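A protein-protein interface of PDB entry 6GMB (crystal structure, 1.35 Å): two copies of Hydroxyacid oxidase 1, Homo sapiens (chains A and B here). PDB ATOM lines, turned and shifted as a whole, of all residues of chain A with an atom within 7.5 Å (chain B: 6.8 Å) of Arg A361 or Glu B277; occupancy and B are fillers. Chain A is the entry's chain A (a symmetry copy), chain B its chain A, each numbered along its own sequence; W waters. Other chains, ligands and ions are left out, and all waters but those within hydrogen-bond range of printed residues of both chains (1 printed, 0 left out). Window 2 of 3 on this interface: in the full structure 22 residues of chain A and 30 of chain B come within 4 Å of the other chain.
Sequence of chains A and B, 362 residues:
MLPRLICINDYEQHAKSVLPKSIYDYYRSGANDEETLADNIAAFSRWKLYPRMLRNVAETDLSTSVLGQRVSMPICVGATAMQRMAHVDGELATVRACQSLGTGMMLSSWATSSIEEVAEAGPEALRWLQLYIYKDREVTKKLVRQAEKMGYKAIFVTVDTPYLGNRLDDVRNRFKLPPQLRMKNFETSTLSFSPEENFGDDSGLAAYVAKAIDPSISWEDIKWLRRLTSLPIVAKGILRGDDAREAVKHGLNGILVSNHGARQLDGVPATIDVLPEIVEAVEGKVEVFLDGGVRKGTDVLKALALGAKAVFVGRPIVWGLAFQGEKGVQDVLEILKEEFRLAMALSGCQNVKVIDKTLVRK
Of the 16 printed residues of chain B, 3 touch a printed residue of chain A.
Hydrophobic or aromatic side chains of chain A within 4 Å of the printed part of chain B: Tyr A50.
Among the printed residues, Asp or Glu carboxylates within 4 Å of a Lys or Arg side-chain nitrogen of the other chain: Arg A361 with Glu B277 (2.7 Å).
Water W1 lies within hydrogen-bond range of OH of Tyr A50 (2.7 Å), OE1 of Glu B277 (2.8 Å) and NH1 of Arg A361 (3.3 Å).
O of Arg A361 sits at hydrogen-bond distance from N of Lys A48 (2.9 Å).
N of Tyr A50 lies within hydrogen-bond range of O of Leu A359 (2.8 Å).
NH1 of Arg A361 sits at hydrogen-bond distance from OH of Tyr A50 (3.4 Å).
The guanidinium group of Arg B240 sits at hydrogen-bond distance from the backbone carbonyl oxygen of Tyr A50 (2.9 Å).
The guanidinium group (NH2) of Arg B240 sits close to the backbone carbonyl oxygen (O) of Thr A358 (3.2 Å).
NH2 of Arg A361 is in salt-bridge range of OE2 of Glu B277 (2.7 Å).
Of the printed residues of chain B, Arg A361 touches Glu B277.
Of the printed residues of chain A, Glu B277 touches Arg A361 (2.7 Å).
Printed residues of chain B within 4 Å of Thr A358: Arg B240 (2.9 Å).
Printed residues of chain A within 4 Å of Arg B240: Tyr A50 (2.9 Å) and Thr A358 (2.9 Å).
Lys A48 touches none of the printed residues of chain B.
Leu A306 touches none of the printed residues of chain B.
Position printed for both chains: 306.
Of the 5 pairs that touch across the chains among the printed residues, none has its exchanged pair printed and touching as well.
O of Leu A49 touches CD of Pro B269, at 3.1 Å.
CZ of Tyr A50 touches CG of Pro B269 (3.4 Å).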
ATOM      1  N   SER A  45     -29.862  -4.762 -14.015  1.00  0.00           N
ATOM      2  CA  SER A  45     -30.885  -5.226 -14.935  1.00  0.00           C
ATOM      3  C   SER A  45     -30.869  -4.400 -16.230  1.00  0.00           C
ATOM      4  O   SER A  45     -31.295  -4.871 -17.277  1.00  0.00           O
ATOM      5  CB  SER A  45     -32.242  -5.200 -14.274  1.00  0.00           C
ATOM      6  OG  SER A  45     -32.257  -5.978 -13.080  1.00  0.00           O
ATOM      7  N   ARG A  46     -30.402  -3.144 -16.162  1.00  0.00           N
ATOM      8  CA  ARG A  46     -30.409  -2.264 -17.338  1.00  0.00           C
ATOM      9  C   ARG A  46     -29.252  -2.581 -18.287  1.00  0.00           C
ATOM     10  O   ARG A  46     -29.318  -2.232 -19.456  1.00  0.00           O
ATOM     11  CB  ARG A  46     -30.327  -0.791 -16.933  1.00  0.00           C
ATOM     12  CG  ARG A  46     -31.551  -0.279 -16.190  1.00  0.00           C
ATOM     13  CD  ARG A  46     -31.487   1.226 -15.975  1.00  0.00           C
ATOM     14  NE  ARG A  46     -30.445   1.644 -15.037  1.00  0.00           N
ATOM     15  CZ  ARG A  46     -30.645   1.956 -13.761  1.00  0.00           C
ATOM     16  NH1 ARG A  46     -31.840   1.794 -13.222  1.00  0.00           N
ATOM     17  NH2 ARG A  46     -29.638   2.403 -13.028  1.00  0.00           N
ATOM     18  N   TRP A  47     -28.194  -3.211 -17.776  1.00  0.00           N
ATOM     19  CA  TRP A  47     -27.095  -3.664 -18.616  1.00  0.00           C
ATOM     20  C   TRP A  47     -27.490  -4.997 -19.247  1.00  0.00           C
ATOM     21  O   TRP A  47     -27.693  -5.974 -18.541  1.00  0.00           O
ATOM     22  CB  TRP A  47     -25.807  -3.794 -17.804  1.00  0.00           C
ATOM     23  CG  TRP A  47     -25.179  -2.488 -17.437  1.00  0.00           C
ATOM     24  CD1 TRP A  47     -25.317  -1.806 -16.265  1.00  0.00           C
ATOM     25  CD2 TRP A  47     -24.308  -1.700 -18.263  1.00  0.00           C
ATOM     26  NE1 TRP A  47     -24.583  -0.653 -16.297  1.00  0.00           N
ATOM     27  CE2 TRP A  47     -23.956  -0.558 -17.512  1.00  0.00           C
ATOM     28  CE3 TRP A  47     -23.783  -1.851 -19.550  1.00  0.00           C
ATOM     29  CZ2 TRP A  47     -23.099   0.419 -18.013  1.00  0.00           C
ATOM     30  CZ3 TRP A  47     -22.953  -0.876 -20.048  1.00  0.00           C
ATOM     31  CH2 TRP A  47     -22.613   0.238 -19.286  1.00  0.00           C
ATOM     32  N   LYS A  48     -27.609  -5.021 -20.570  1.00  0.00           N
ATOM     33  CA  LYS A  48     -28.068  -6.212 -21.265  1.00  0.00           C
ATOM     34  C   LYS A  48     -26.870  -6.993 -21.816  1.00  0.00           C
ATOM     35  O   LYS A  48     -25.848  -6.427 -22.180  1.00  0.00           O
ATOM     36  CB  LYS A  48     -29.059  -5.851 -22.372  1.00  0.00           C
ATOM     37  CG  LYS A  48     -30.321  -5.149 -21.880  1.00  0.00           C
ATOM     38  CD  LYS A  48     -31.170  -6.014 -20.957  1.00  0.00           C
ATOM     39  CE  LYS A  48     -32.434  -5.367 -20.429  1.00  0.00           C
ATOM     40  NZ  LYS A  48     -33.212  -6.335 -19.616  1.00  0.00           N
ATOM     41  N   LEU A  49     -27.036  -8.314 -21.871  1.00  0.00           N
ATOM     42  CA  LEU A  49     -26.002  -9.237 -22.322  1.00  0.00           C
ATOM     43  C   LEU A  49     -26.220  -9.619 -23.788  1.00  0.00           C
ATOM     44  O   LEU A  49     -27.346  -9.880 -24.223  1.00  0.00           O
ATOM     45  CB  LEU A  49     -26.035 -10.484 -21.437  1.00  0.00           C
ATOM     46  CG  LEU A  49     -25.471 -10.287 -20.032  1.00  0.00           C
ATOM     47  CD1 LEU A  49     -25.926 -11.406 -19.109  1.00  0.00           C
ATOM     48  CD2 LEU A  49     -23.952 -10.206 -20.067  1.00  0.00           C
ATOM     49  N   TYR A  50     -25.100  -9.709 -24.509  1.00  0.00           N
ATOM     50  CA  TYR A  50     -25.049 -10.025 -25.926  1.00  0.00           C
ATOM     51  C   TYR A  50     -24.195 -11.270 -26.100  1.00  0.00           C
ATOM     52  O   TYR A  50     -23.014 -11.193 -26.432  1.00  0.00           O
ATOM     53  CB  TYR A  50     -24.522  -8.826 -26.712  1.00  0.00           C
ATOM     54  CG  TYR A  50     -25.529  -7.711 -26.765  1.00  0.00           C
ATOM     55  CD1 TYR A  50     -25.735  -6.891 -25.670  1.00  0.00           C
ATOM     56  CD2 TYR A  50     -26.322  -7.517 -27.885  1.00  0.00           C
ATOM     57  CE1 TYR A  50     -26.715  -5.916 -25.679  1.00  0.00           C
ATOM     58  CE2 TYR A  50     -27.295  -6.532 -27.916  1.00  0.00           C
ATOM     59  CZ  TYR A  50     -27.491  -5.729 -26.806  1.00  0.00           C
ATOM     60  OH  TYR A  50     -28.433  -4.739 -26.808  1.00  0.00           O
ATOM     61  N   LEU A 306     -17.377  -5.023 -17.813  1.00  0.00           N
ATOM     62  CA  LEU A 306     -17.132  -3.573 -17.722  1.00  0.00           C
ATOM     63  C   LEU A 306     -15.777  -3.261 -17.068  1.00  0.00           C
ATOM     64  O   LEU A 306     -15.457  -2.090 -16.869  1.00  0.00           O
ATOM     65  CB  LEU A 306     -18.292  -2.918 -16.963  1.00  0.00           C
ATOM     66  CG  LEU A 306     -19.609  -2.876 -17.735  1.00  0.00           C
ATOM     67  CD1 LEU A 306     -20.724  -2.357 -16.852  1.00  0.00           C
ATOM     68  CD2 LEU A 306     -19.493  -2.046 -19.004  1.00  0.00           C
ATOM     69  N   LYS A 357     -15.933  -6.185 -23.254  1.00  0.00           N
ATOM     70  CA  LYS A 357     -16.926  -5.099 -23.195  1.00  0.00           C
ATOM     71  C   LYS A 357     -18.051  -5.310 -24.219  1.00  0.00           C
ATOM     72  O   LYS A 357     -19.125  -4.763 -24.055  1.00  0.00           O
ATOM     73  CB  LYS A 357     -16.279  -3.735 -23.462  1.00  0.00           C
ATOM     74  N   THR A 358     -17.821  -6.082 -25.289  1.00  0.00           N
ATOM     75  CA  THR A 358     -18.853  -6.279 -26.304  1.00  0.00           C
ATOM     76  C   THR A 358     -19.986  -7.178 -25.774  1.00  0.00           C
ATOM     77  O   THR A 358     -21.066  -7.271 -26.372  1.00  0.00           O
ATOM     78  CB  THR A 358     -18.218  -6.820 -27.588  1.00  0.00           C
ATOM     79  OG1 THR A 358     -18.743  -6.105 -28.706  1.00  0.00           O
ATOM     80  CG2 THR A 358     -18.436  -8.304 -27.738  1.00  0.00           C
ATOM     81  N   LEU A 359     -19.749  -7.836 -24.637  1.00  0.00           N
ATOM     82  CA  LEU A 359     -20.782  -8.669 -24.053  1.00  0.00           C
ATOM     83  C   LEU A 359     -21.935  -7.839 -23.479  1.00  0.00           C
ATOM     84  O   LEU A 359     -22.995  -8.411 -23.213  1.00  0.00           O
ATOM     85  CB  LEU A 359     -20.183  -9.546 -22.957  1.00  0.00           C
ATOM     86  CG  LEU A 359     -19.429 -10.780 -23.432  1.00  0.00           C
ATOM     87  CD1 LEU A 359     -18.789 -11.482 -22.250  1.00  0.00           C
ATOM     88  CD2 LEU A 359     -20.343 -11.742 -24.180  1.00  0.00           C
ATOM     89  N   VAL A 360     -21.738  -6.538 -23.228  1.00  0.00           N
ATOM     90  CA  VAL A 360     -22.786  -5.758 -22.556  1.00  0.00           C
ATOM     91  C   VAL A 360     -23.081  -4.462 -23.311  1.00  0.00           C
ATOM     92  O   VAL A 360     -22.205  -3.876 -23.956  1.00  0.00           O
ATOM     93  CB  VAL A 360     -22.448  -5.458 -21.087  1.00  0.00           C
ATOM     94  CG1 VAL A 360     -22.408  -6.728 -20.260  1.00  0.00           C
ATOM     95  CG2 VAL A 360     -21.172  -4.648 -20.940  1.00  0.00           C
ATOM     96  N   ARG A 361     -24.325  -3.997 -23.162  1.00  0.00           N
ATOM     97  CA  ARG A 361     -24.762  -2.691 -23.672  1.00  0.00           C
ATOM     98  C   ARG A 361     -25.850  -2.173 -22.732  1.00  0.00           C
ATOM     99  O   ARG A 361     -26.725  -2.938 -22.355  1.00  0.00           O
ATOM    100  CB  ARG A 361     -25.306  -2.838 -25.101  1.00  0.00           C
ATOM    101  CG  ARG A 361     -25.416  -1.566 -25.929  1.00  0.00           C
ATOM    102  CD  ARG A 361     -26.140  -1.842 -27.245  1.00  0.00           C
ATOM    103  NE  ARG A 361     -25.524  -2.867 -28.091  1.00  0.00           N
ATOM    104  CZ  ARG A 361     -26.085  -3.383 -29.189  1.00  0.00           C
ATOM    105  NH1 ARG A 361     -27.313  -3.038 -29.535  1.00  0.00           N
ATOM    106  NH2 ARG A 361     -25.428  -4.258 -29.933  1.00  0.00           N
ATOM    107  N   LYS A 362     -25.806  -0.887 -22.375  1.00  0.00           N
ATOM    108  CA  LYS A 362     -26.827  -0.338 -21.473  1.00  0.00           C
ATOM    109  C   LYS A 362     -27.993   0.194 -22.306  1.00  0.00           C
ATOM    110  O   LYS A 362     -27.786   0.929 -23.259  1.00  0.00           O
ATOM    111  CB  LYS A 362     -26.267   0.754 -20.556  1.00  0.00           C
ATOM    112  CG  LYS A 362     -27.259   1.274 -19.521  1.00  0.00           C
ATOM    113  CD  LYS A 362     -26.625   1.887 -18.288  1.00  0.00           C
ATOM    114  CE  LYS A 362     -25.589   2.945 -18.601  1.00  0.00           C
ATOM    115  NZ  LYS A 362     -25.376   3.854 -17.447  1.00  0.00           N
ATOM    116  N   LEU B 239     -28.262 -13.850 -31.358  1.00  0.00           N
ATOM    117  CA  LEU B 239     -28.629 -12.538 -30.830  1.00  0.00           C
ATOM    118  C   LEU B 239     -27.635 -11.441 -31.226  1.00  0.00           C
ATOM    119  O   LEU B 239     -27.902 -10.299 -30.927  1.00  0.00           O
ATOM    120  CB  LEU B 239     -28.738 -12.634 -29.303  1.00  0.00           C
ATOM    121  CG  LEU B 239     -29.901 -13.482 -28.790  1.00  0.00           C
ATOM    122  CD1 LEU B 239     -29.792 -13.677 -27.290  1.00  0.00           C
ATOM    123  CD2 LEU B 239     -31.252 -12.876 -29.156  1.00  0.00           C
ATOM    124  N   ARG B 240     -26.519 -11.788 -31.874  1.00  0.00           N
ATOM    125  CA  ARG B 240     -25.488 -10.835 -32.270  1.00  0.00           C
ATOM    126  C   ARG B 240     -25.337 -10.814 -33.795  1.00  0.00           C
ATOM    127  O   ARG B 240     -25.346 -11.855 -34.452  1.00  0.00           O
ATOM    128  CB  ARG B 240     -24.127 -11.223 -31.689  1.00  0.00           C
ATOM    129  CG  ARG B 240     -24.009 -11.153 -30.175  1.00  0.00           C
ATOM    130  CD  ARG B 240     -22.697 -11.746 -29.696  1.00  0.00           C
ATOM    131  NE  ARG B 240     -21.544 -10.998 -30.170  1.00  0.00           N
ATOM    132  CZ  ARG B 240     -20.798 -10.181 -29.443  1.00  0.00           C
ATOM    133  NH1 ARG B 240     -19.768  -9.590 -30.018  1.00  0.00           N
ATOM    134  NH2 ARG B 240     -21.060  -9.959 -28.164  1.00  0.00           N
ATOM    135  N   GLY B 241     -25.108  -9.616 -34.332  1.00  0.00           N
ATOM    136  CA  GLY B 241     -24.844  -9.445 -35.748  1.00  0.00           C
ATOM    137  C   GLY B 241     -23.610 -10.202 -36.226  1.00  0.00           C
ATOM    138  O   GLY B 241     -23.620 -10.777 -37.324  1.00  0.00           O
ATOM    139  N   ALA B 244     -24.496 -13.733 -36.640  1.00  0.00           N
ATOM    140  CA  ALA B 244     -25.353 -13.867 -37.807  1.00  0.00           C
ATOM    141  C   ALA B 244     -24.516 -13.910 -39.094  1.00  0.00           C
ATOM    142  O   ALA B 244     -24.774 -14.721 -39.980  1.00  0.00           O
ATOM    143  CB  ALA B 244     -26.361 -12.744 -37.841  1.00  0.00           C
ATOM    144  N   PRO B 269     -31.303  -8.986 -24.491  1.00  0.00           N
ATOM    145  CA  PRO B 269     -32.389  -8.142 -24.970  1.00  0.00           C
ATOM    146  C   PRO B 269     -33.578  -8.957 -25.486  1.00  0.00           C
ATOM    147  O   PRO B 269     -33.469 -10.158 -25.766  1.00  0.00           O
ATOM    148  CB  PRO B 269     -31.780  -7.363 -26.140  1.00  0.00           C
ATOM    149  CG  PRO B 269     -30.299  -7.529 -25.965  1.00  0.00           C
ATOM    150  CD  PRO B 269     -30.109  -8.891 -25.341  1.00  0.00           C
ATOM    151  N   ASP B 273     -36.085  -6.266 -30.241  1.00  0.00           N
ATOM    152  CA  ASP B 273     -35.104  -5.181 -30.161  1.00  0.00           C
ATOM    153  C   ASP B 273     -33.802  -5.531 -30.893  1.00  0.00           C
ATOM    154  O   ASP B 273     -33.138  -4.623 -31.394  1.00  0.00           O
ATOM    155  CB  ASP B 273     -34.827  -4.789 -28.711  1.00  0.00           C
ATOM    156  CG  ASP B 273     -35.939  -3.971 -28.084  1.00  0.00           C
ATOM    157  OD1 ASP B 273     -36.763  -3.414 -28.849  1.00  0.00           O
ATOM    158  OD2 ASP B 273     -35.971  -3.887 -26.840  1.00  0.00           O
ATOM    159  N   VAL B 274     -33.401  -6.806 -30.923  1.00  0.00           N
ATOM    160  CA  VAL B 274     -32.160  -7.154 -31.634  1.00  0.00           C
ATOM    161  C   VAL B 274     -32.440  -7.479 -33.106  1.00  0.00           C
ATOM    162  O   VAL B 274     -31.513  -7.450 -33.918  1.00  0.00           O
ATOM    163  CB  VAL B 274     -31.358  -8.277 -30.962  1.00  0.00           C
ATOM    164  CG1 VAL B 274     -30.845  -7.876 -29.596  1.00  0.00           C
ATOM    165  CG2 VAL B 274     -32.134  -9.558 -30.886  1.00  0.00           C
ATOM    166  N   LEU B 275     -33.701  -7.751 -33.465  1.00  0.00           N
ATOM    167  CA  LEU B 275     -34.027  -8.113 -34.846  1.00  0.00           C
ATOM    168  C   LEU B 275     -33.438  -7.119 -35.854  1.00  0.00           C
ATOM    169  O   LEU B 275     -32.827  -7.556 -36.835  1.00  0.00           O
ATOM    170  CB  LEU B 275     -35.541  -8.247 -34.985  1.00  0.00           C
ATOM    171  CG  LEU B 275     -36.054  -8.508 -36.397  1.00  0.00           C
ATOM    172  CD1 LEU B 275     -35.562  -9.840 -36.935  1.00  0.00           C
ATOM    173  CD2 LEU B 275     -37.570  -8.441 -36.425  1.00  0.00           C
ATOM    174  N   PRO B 276     -33.582  -5.777 -35.706  1.00  0.00           N
ATOM    175  CA  PRO B 276     -33.039  -4.869 -36.719  1.00  0.00           C
ATOM    176  C   PRO B 276     -31.532  -5.048 -36.967  1.00  0.00           C
ATOM    177  O   PRO B 276     -31.106  -4.979 -38.120  1.00  0.00           O
ATOM    178  CB  PRO B 276     -33.311  -3.458 -36.185  1.00  0.00           C
ATOM    179  CG  PRO B 276     -34.452  -3.644 -35.215  1.00  0.00           C
ATOM    180  CD  PRO B 276     -34.313  -5.047 -34.660  1.00  0.00           C
ATOM    181  N   GLU B 277     -30.737  -5.246 -35.904  1.00  0.00           N
ATOM    182  CA  GLU B 277     -29.292  -5.430 -36.040  1.00  0.00           C
ATOM    183  C   GLU B 277     -28.998  -6.674 -36.885  1.00  0.00           C
ATOM    184  O   GLU B 277     -28.100  -6.678 -37.705  1.00  0.00           O
ATOM    185  CB  GLU B 277     -28.631  -5.599 -34.669  1.00  0.00           C
ATOM    186  CG  GLU B 277     -28.676  -4.359 -33.798  1.00  0.00           C
ATOM    187  CD  GLU B 277     -28.215  -4.585 -32.366  1.00  0.00           C
ATOM    188  OE1 GLU B 277     -29.017  -5.086 -31.531  1.00  0.00           O
ATOM    189  OE2 GLU B 277     -27.038  -4.278 -32.089  1.00  0.00           O
ATOM    190  N   ILE B 278     -29.762  -7.737 -36.651  1.00  0.00           N
ATOM    191  CA  ILE B 278     -29.521  -8.999 -37.352  1.00  0.00           C
ATOM    192  C   ILE B 278     -29.931  -8.870 -38.823  1.00  0.00           C
ATOM    193  O   ILE B 278     -29.198  -9.313 -39.714  1.00  0.00           O
ATOM    194  CB  ILE B 278     -30.242 -10.177 -36.676  1.00  0.00           C
ATOM    195  CG1 ILE B 278     -29.867 -10.304 -35.201  1.00  0.00           C
ATOM    196  CG2 ILE B 278     -29.993 -11.468 -37.438  1.00  0.00           C
ATOM    197  CD1 ILE B 278     -28.403 -10.412 -34.950  1.00  0.00           C
ATOM    198  N   VAL B 279     -31.099  -8.273 -39.075  1.00  0.00           N
ATOM    199  CA  VAL B 279     -31.538  -8.038 -40.449  1.00  0.00           C
ATOM    200  C   VAL B 279     -30.467  -7.231 -41.200  1.00  0.00           C
ATOM    201  O   VAL B 279     -30.095  -7.578 -42.317  1.00  0.00           O
ATOM    202  CB  VAL B 279     -32.915  -7.352 -40.477  1.00  0.00           C
ATOM    203  CG1 VAL B 279     -33.290  -6.860 -41.868  1.00  0.00           C
ATOM    204  CG2 VAL B 279     -33.978  -8.297 -39.944  1.00  0.00           C
ATOM    205  N   GLU B 280     -29.950  -6.171 -40.578  1.00  0.00           N
ATOM    206  CA  GLU B 280     -28.925  -5.345 -41.226  1.00  0.00           C
ATOM    207  C   GLU B 280     -27.664  -6.182 -41.492  1.00  0.00           C
ATOM    208  O   GLU B 280     -27.081  -6.103 -42.567  1.00  0.00           O
ATOM    209  CB  GLU B 280     -28.608  -4.108 -40.385  1.00  0.00           C
ATOM    210  CG  GLU B 280     -27.557  -3.199 -41.014  1.00  0.00           C
ATOM    211  CD  GLU B 280     -27.195  -1.952 -40.224  1.00  0.00           C
ATOM    212  OE1 GLU B 280     -27.331  -1.969 -38.985  1.00  0.00           O
ATOM    213  OE2 GLU B 280     -26.761  -0.970 -40.852  1.00  0.00           O
ATOM    214  N   ALA B 281     -27.247  -6.985 -40.508  1.00  0.00           N
ATOM    215  CA  ALA B 281     -25.984  -7.721 -40.586  1.00  0.00           C
ATOM    216  C   ALA B 281     -25.988  -8.736 -41.736  1.00  0.00           C
ATOM    217  O   ALA B 281     -24.935  -8.954 -42.335  1.00  0.00           O
ATOM    218  CB  ALA B 281     -25.699  -8.406 -39.274  1.00  0.00           C
ATOM    219  N   VAL B 282     -27.132  -9.369 -42.036  1.00  0.00           N
ATOM    220  CA  VAL B 282     -27.099 -10.461 -43.030  1.00  0.00           C
ATOM    221  C   VAL B 282     -27.292  -9.939 -44.460  1.00  0.00           C
ATOM    222  O   VAL B 282     -27.126 -10.707 -45.398  1.00  0.00           O
ATOM    223  CB  VAL B 282     -28.089 -11.590 -42.717  1.00  0.00           C
ATOM    224  CG1 VAL B 282     -27.879 -12.158 -41.331  1.00  0.00           C
ATOM    225  CG2 VAL B 282     -29.523 -11.159 -42.902  1.00  0.00           C
ATOM    226  N   LEU B 306     -39.927  -4.793 -39.268  1.00  0.00           N
ATOM    227  CA  LEU B 306     -38.494  -4.690 -38.945  1.00  0.00           C
ATOM    228  C   LEU B 306     -37.660  -5.734 -39.705  1.00  0.00           C
ATOM    229  O   LEU B 306     -36.450  -5.810 -39.495  1.00  0.00           O
ATOM    230  CB  LEU B 306     -38.313  -4.815 -37.429  1.00  0.00           C
ATOM    231  CG  LEU B 306     -38.811  -3.611 -36.631  1.00  0.00           C
ATOM    232  CD1 LEU B 306     -38.734  -3.892 -35.145  1.00  0.00           C
ATOM    233  CD2 LEU B 306     -38.044  -2.347 -36.983  1.00  0.00           C
HETATM  234  O   HOH W   1     -30.115  -4.622 -28.949  1.00  0.00           O
